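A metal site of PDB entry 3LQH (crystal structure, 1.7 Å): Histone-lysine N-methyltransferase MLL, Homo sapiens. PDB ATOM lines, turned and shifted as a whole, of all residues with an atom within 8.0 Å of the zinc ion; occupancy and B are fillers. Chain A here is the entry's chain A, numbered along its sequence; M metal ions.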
ATOM      1  N   PHE A   4       2.719   3.892 -30.882  1.00  0.00           N
ATOM      2  CA  PHE A   4       2.693   3.031 -29.703  1.00  0.00           C
ATOM      3  C   PHE A   4       1.774   3.524 -28.595  1.00  0.00           C
ATOM      4  O   PHE A   4       1.676   4.730 -28.342  1.00  0.00           O
ATOM      5  CB  PHE A   4       4.106   2.929 -29.121  1.00  0.00           C
ATOM      6  CG  PHE A   4       5.105   2.279 -30.030  1.00  0.00           C
ATOM      7  CD1 PHE A   4       5.448   0.937 -29.873  1.00  0.00           C
ATOM      8  CD2 PHE A   4       5.705   3.011 -31.053  1.00  0.00           C
ATOM      9  CE1 PHE A   4       6.373   0.336 -30.719  1.00  0.00           C
ATOM     10  CE2 PHE A   4       6.639   2.414 -31.903  1.00  0.00           C
ATOM     11  CZ  PHE A   4       6.973   1.076 -31.736  1.00  0.00           C
ATOM     12  N   CYS A   5       1.098   2.592 -27.925  1.00  0.00           N
ATOM     13  CA  CYS A   5       0.251   2.947 -26.792  1.00  0.00           C
ATOM     14  C   CYS A   5       1.212   3.317 -25.671  1.00  0.00           C
ATOM     15  O   CYS A   5       2.082   2.524 -25.303  1.00  0.00           O
ATOM     16  CB  CYS A   5      -0.604   1.762 -26.356  1.00  0.00           C
ATOM     17  SG  CYS A   5      -1.399   2.015 -24.751  1.00  0.00           S
ATOM     18  N   PRO A   6       1.064   4.509 -25.097  1.00  0.00           N
ATOM     19  CA  PRO A   6       1.960   4.930 -24.006  1.00  0.00           C
ATOM     20  C   PRO A   6       1.855   4.183 -22.689  1.00  0.00           C
ATOM     21  O   PRO A   6       2.710   4.337 -21.811  1.00  0.00           O
ATOM     22  CB  PRO A   6       1.644   6.422 -23.863  1.00  0.00           C
ATOM     23  CG  PRO A   6       0.190   6.474 -24.220  1.00  0.00           C
ATOM     24  CD  PRO A   6       0.108   5.572 -25.428  1.00  0.00           C
ATOM     25  N   LEU A   7       0.881   3.328 -22.532  1.00  0.00           N
ATOM     26  CA  LEU A   7       0.716   2.618 -21.365  1.00  0.00           C
ATOM     27  C   LEU A   7       1.084   1.177 -21.353  1.00  0.00           C
ATOM     28  O   LEU A   7       0.904   0.549 -20.405  1.00  0.00           O
ATOM     29  CB  LEU A   7      -0.754   2.759 -20.864  1.00  0.00           C
ATOM     30  CG  LEU A   7      -1.255   4.102 -20.523  1.00  0.00           C
ATOM     31  CD1 LEU A   7      -2.678   4.063 -20.133  1.00  0.00           C
ATOM     32  CD2 LEU A   7      -0.563   4.581 -19.523  1.00  0.00           C
ATOM     33  N   CYS A   8       1.574   0.681 -22.428  1.00  0.00           N
ATOM     34  CA  CYS A   8       2.059  -0.686 -22.512  1.00  0.00           C
ATOM     35  C   CYS A   8       3.267  -0.736 -23.449  1.00  0.00           C
ATOM     36  O   CYS A   8       3.945  -1.759 -23.556  1.00  0.00           O
ATOM     37  CB  CYS A   8       0.964  -1.635 -23.015  1.00  0.00           C
ATOM     38  SG  CYS A   8       0.417  -1.351 -24.723  1.00  0.00           S
ATOM     39  N   ASP A   9       3.503   0.364 -24.069  1.00  0.00           N
ATOM     40  CA  ASP A   9       4.533   0.511 -25.012  1.00  0.00           C
ATOM     41  C   ASP A   9       4.518  -0.381 -26.214  1.00  0.00           C
ATOM     42  O   ASP A   9       5.495  -0.640 -26.750  1.00  0.00           O
ATOM     43  CB  ASP A   9       5.874   0.323 -24.348  1.00  0.00           C
ATOM     44  CG  ASP A   9       6.339   1.543 -23.632  1.00  0.00           C
ATOM     45  OD1 ASP A   9       5.950   2.518 -23.962  1.00  0.00           O
ATOM     46  OD2 ASP A   9       7.097   1.434 -22.698  1.00  0.00           O
ATOM     47  N   LYS A  10       3.385  -0.902 -26.524  1.00  0.00           N
ATOM     48  CA  LYS A  10       3.197  -1.805 -27.658  1.00  0.00           C
ATOM     49  C   LYS A  10       2.680  -1.035 -28.858  1.00  0.00           C
ATOM     50  O   LYS A  10       1.819  -0.163 -28.720  1.00  0.00           O
ATOM     51  CB  LYS A  10       2.208  -2.920 -27.292  1.00  0.00           C
ATOM     52  CG  LYS A  10       2.596  -3.716 -26.068  1.00  0.00           C
ATOM     53  CD  LYS A  10       3.979  -4.324 -26.217  1.00  0.00           C
ATOM     54  CE  LYS A  10       4.064  -5.261 -27.409  1.00  0.00           C
ATOM     55  NZ  LYS A  10       5.439  -5.796 -27.596  1.00  0.00           N
ATOM     56  N   CYS A  11       3.220  -1.340 -30.030  1.00  0.00           N
ATOM     57  CA  CYS A  11       2.801  -0.699 -31.275  1.00  0.00           C
ATOM     58  C   CYS A  11       1.403  -1.192 -31.597  1.00  0.00           C
ATOM     59  O   CYS A  11       1.123  -2.384 -31.498  1.00  0.00           O
ATOM     60  CB  CYS A  11       3.774  -1.074 -32.395  1.00  0.00           C
ATOM     61  SG  CYS A  11       3.357  -0.416 -34.027  1.00  0.00           S
ATOM     62  N   TYR A  12       0.515  -0.277 -31.983  1.00  0.00           N
ATOM     63  CA  TYR A  12      -0.851  -0.668 -32.301  1.00  0.00           C
ATOM     64  C   TYR A  12      -1.201  -0.557 -33.787  1.00  0.00           C
ATOM     65  O   TYR A  12      -2.358  -0.688 -34.167  1.00  0.00           O
ATOM     66  CB  TYR A  12      -1.846   0.134 -31.444  1.00  0.00           C
ATOM     67  CG  TYR A  12      -1.743   1.637 -31.557  1.00  0.00           C
ATOM     68  CD1 TYR A  12      -2.260   2.317 -32.669  1.00  0.00           C
ATOM     69  CD2 TYR A  12      -1.138   2.385 -30.550  1.00  0.00           C
ATOM     70  CE1 TYR A  12      -2.184   3.705 -32.756  1.00  0.00           C
ATOM     71  CE2 TYR A  12      -1.057   3.775 -30.624  1.00  0.00           C
ATOM     72  CZ  TYR A  12      -1.578   4.431 -31.739  1.00  0.00           C
ATOM     73  OH  TYR A  12      -1.496   5.806 -31.796  1.00  0.00           O
ATOM     74  N   ASP A  15      -2.926  -3.541 -34.866  1.00  0.00           N
ATOM     75  CA  ASP A  15      -4.055  -3.931 -34.028  1.00  0.00           C
ATOM     76  C   ASP A  15      -5.303  -4.126 -34.873  1.00  0.00           C
ATOM     77  O   ASP A  15      -5.627  -3.293 -35.725  1.00  0.00           O
ATOM     78  CB  ASP A  15      -4.326  -2.854 -32.974  1.00  0.00           C
ATOM     79  CG  ASP A  15      -3.534  -3.075 -31.712  1.00  0.00           C
ATOM     80  OD1 ASP A  15      -2.355  -3.479 -31.813  1.00  0.00           O
ATOM     81  OD2 ASP A  15      -4.085  -2.851 -30.615  1.00  0.00           O
ATOM     82  N   SER A  19      -9.602  -4.406 -31.176  1.00  0.00           N
ATOM     83  CA  SER A  19      -8.824  -3.714 -30.159  1.00  0.00           C
ATOM     84  C   SER A  19      -9.480  -2.398 -29.747  1.00  0.00           C
ATOM     85  O   SER A  19      -9.402  -1.404 -30.464  1.00  0.00           O
ATOM     86  CB  SER A  19      -7.410  -3.453 -30.683  1.00  0.00           C
ATOM     87  OG  SER A  19      -6.597  -2.876 -29.685  1.00  0.00           O
ATOM     88  N   LYS A  20     -10.129  -2.392 -28.586  1.00  0.00           N
ATOM     89  CA  LYS A  20     -10.790  -1.182 -28.112  1.00  0.00           C
ATOM     90  C   LYS A  20      -9.777  -0.174 -27.559  1.00  0.00           C
ATOM     91  O   LYS A  20      -8.984  -0.482 -26.669  1.00  0.00           O
ATOM     92  CB  LYS A  20     -11.843  -1.519 -27.059  1.00  0.00           C
ATOM     93  CG  LYS A  20     -11.359  -2.385 -25.917  1.00  0.00           C
ATOM     94  CD  LYS A  20     -12.485  -3.278 -25.401  1.00  0.00           C
ATOM     95  CE  LYS A  20     -13.694  -2.465 -24.964  1.00  0.00           C
ATOM     96  NZ  LYS A  20     -13.332  -1.520 -23.872  1.00  0.00           N
ATOM     97  N   MET A  21      -9.818   1.034 -28.116  1.00  0.00           N
ATOM     98  CA  MET A  21      -8.906   2.093 -27.716  1.00  0.00           C
ATOM     99  C   MET A  21      -9.637   3.428 -27.681  1.00  0.00           C
ATOM    100  O   MET A  21     -10.755   3.545 -28.162  1.00  0.00           O
ATOM    101  CB  MET A  21      -7.732   2.196 -28.709  1.00  0.00           C
ATOM    102  CG  MET A  21      -7.017   0.889 -29.022  1.00  0.00           C
ATOM    103  SD  MET A  21      -5.632   1.084 -30.175  1.00  0.00           S
ATOM    104  CE  MET A  21      -4.358   1.693 -29.043  1.00  0.00           C
ATOM    105  N   TRP A  30      -3.388   7.006 -29.660  1.00  0.00           N
ATOM    106  CA  TRP A  30      -4.401   6.096 -29.134  1.00  0.00           C
ATOM    107  C   TRP A  30      -3.896   5.283 -27.947  1.00  0.00           C
ATOM    108  O   TRP A  30      -2.703   4.993 -27.843  1.00  0.00           O
ATOM    109  CB  TRP A  30      -4.907   5.165 -30.232  1.00  0.00           C
ATOM    110  CG  TRP A  30      -5.654   5.888 -31.309  1.00  0.00           C
ATOM    111  CD1 TRP A  30      -5.112   6.629 -32.329  1.00  0.00           C
ATOM    112  CD2 TRP A  30      -7.073   6.009 -31.425  1.00  0.00           C
ATOM    113  NE1 TRP A  30      -6.119   7.198 -33.085  1.00  0.00           N
ATOM    114  CE2 TRP A  30      -7.332   6.833 -32.554  1.00  0.00           C
ATOM    115  CE3 TRP A  30      -8.159   5.506 -30.699  1.00  0.00           C
ATOM    116  CZ2 TRP A  30      -8.623   7.157 -32.961  1.00  0.00           C
ATOM    117  CZ3 TRP A  30      -9.450   5.830 -31.106  1.00  0.00           C
ATOM    118  CH2 TRP A  30      -9.668   6.646 -32.225  1.00  0.00           C
ATOM    119  N   VAL A  31      -4.812   4.936 -27.045  1.00  0.00           N
ATOM    120  CA  VAL A  31      -4.492   4.182 -25.841  1.00  0.00           C
ATOM    121  C   VAL A  31      -5.462   3.004 -25.661  1.00  0.00           C
ATOM    122  O   VAL A  31      -6.674   3.173 -25.809  1.00  0.00           O
ATOM    123  CB  VAL A  31      -4.603   5.096 -24.592  1.00  0.00           C
ATOM    124  CG1 VAL A  31      -4.287   4.318 -23.331  1.00  0.00           C
ATOM    125  CG2 VAL A  31      -3.679   6.295 -24.752  1.00  0.00           C
ATOM    126  N   HIS A  32      -4.932   1.840 -25.351  1.00  0.00           N
ATOM    127  CA  HIS A  32      -5.756   0.725 -25.087  1.00  0.00           C
ATOM    128  C   HIS A  32      -6.644   0.885 -23.867  1.00  0.00           C
ATOM    129  O   HIS A  32      -6.236   1.286 -22.940  1.00  0.00           O
ATOM    130  CB  HIS A  32      -5.092  -0.602 -24.996  1.00  0.00           C
ATOM    131  CG  HIS A  32      -4.231  -0.975 -26.169  1.00  0.00           C
ATOM    132  ND1 HIS A  32      -2.912  -0.939 -26.102  1.00  0.00           N
ATOM    133  CD2 HIS A  32      -4.477  -1.561 -27.321  1.00  0.00           C
ATOM    134  CE1 HIS A  32      -2.351  -1.408 -27.144  1.00  0.00           C
ATOM    135  NE2 HIS A  32      -3.286  -1.801 -27.931  1.00  0.00           N
ATOM    136  N   SER A  33      -7.895   0.449 -24.021  1.00  0.00           N
ATOM    137  CA  SER A  33      -8.799   0.564 -22.887  1.00  0.00           C
ATOM    138  C   SER A  33      -8.252  -0.302 -21.759  1.00  0.00           C
ATOM    139  O   SER A  33      -8.264   0.103 -20.592  1.00  0.00           O
ATOM    140  CB  SER A  33     -10.193   0.071 -23.286  1.00  0.00           C
ATOM    141  OG  SER A  33     -11.089   0.173 -22.198  1.00  0.00           O
ATOM    142  N   LYS A  34      -7.758  -1.489 -22.113  1.00  0.00           N
ATOM    143  CA  LYS A  34      -7.200  -2.444 -21.157  1.00  0.00           C
ATOM    144  C   LYS A  34      -6.002  -1.906 -20.374  1.00  0.00           C
ATOM    145  O   LYS A  34      -5.734  -2.371 -19.261  1.00  0.00           O
ATOM    146  CB  LYS A  34      -6.789  -3.728 -21.874  1.00  0.00           C
ATOM    147  CG  LYS A  34      -7.932  -4.684 -22.187  1.00  0.00           C
ATOM    148  CD  LYS A  34      -8.196  -5.620 -21.023  1.00  0.00           C
ATOM    149  CE  LYS A  34      -7.022  -6.558 -20.798  1.00  0.00           C
ATOM    150  NZ  LYS A  34      -7.229  -7.488 -19.654  1.00  0.00           N
ATOM    151  N   CYS A  35      -5.286  -0.942 -20.941  1.00  0.00           N
ATOM    152  CA  CYS A  35      -4.112  -0.378 -20.282  1.00  0.00           C
ATOM    153  C   CYS A  35      -4.441   0.781 -19.356  1.00  0.00           C
ATOM    154  O   CYS A  35      -3.602   1.229 -18.589  1.00  0.00           O
ATOM    155  CB  CYS A  35      -3.085   0.062 -21.333  1.00  0.00           C
ATOM    156  SG  CYS A  35      -2.558  -1.281 -22.391  1.00  0.00           S
ATOM    157  N   GLU A  36      -5.662   1.228 -19.382  1.00  0.00           N
ATOM    158  CA  GLU A  36      -6.091   2.317 -18.607  1.00  0.00           C
ATOM    159  C   GLU A  36      -7.046   1.877 -17.400  1.00  0.00           C
ATOM    160  O   GLU A  36      -7.569   0.917 -17.410  1.00  0.00           O
ATOM    161  CB  GLU A  36      -6.772   3.317 -19.513  1.00  0.00           C
ATOM    162  CG  GLU A  36      -7.141   4.651 -19.020  1.00  0.00           C
ATOM    163  CD  GLU A  36      -5.983   5.577 -18.580  1.00  0.00           C
ATOM    164  OE1 GLU A  36      -5.516   6.347 -19.299  1.00  0.00           O
ATOM    165  OE2 GLU A  36      -5.788   5.509 -17.363  1.00  0.00           O
HETATM  166 ZN    ZN M   1      -1.633  -0.319 -24.310  1.00  0.00          ZN
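ND1 of His 32 is bound to the zinc ion, at 2.3 Å. The zinc ion is bound by SG of Cys 8 (2.3 Å). The zinc ion is bound by the side-chain sulfur (SG) of Cys 35 (2.3 Å). The zinc ion is bound by SG of Cys 5 (2.4 Å).
The side-chain carboxylate (OD2) of Asp 15 sits at hydrogen-bond distance from a ring nitrogen (NE2) of His 32, 3.0 Å away. The side-chain sulfur of Cys 8 lies close to the backbone NH of Lys 10 (3.5 Å). The side-chain sulfur of Cys 5 lies close to the backbone NH of Leu 7 (3.4 Å). The backbone carbonyl oxygen (O) of Lys 10 is in hydrogen-bond range of the backbone NH (N) of Cys 5 (3.0 Å).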
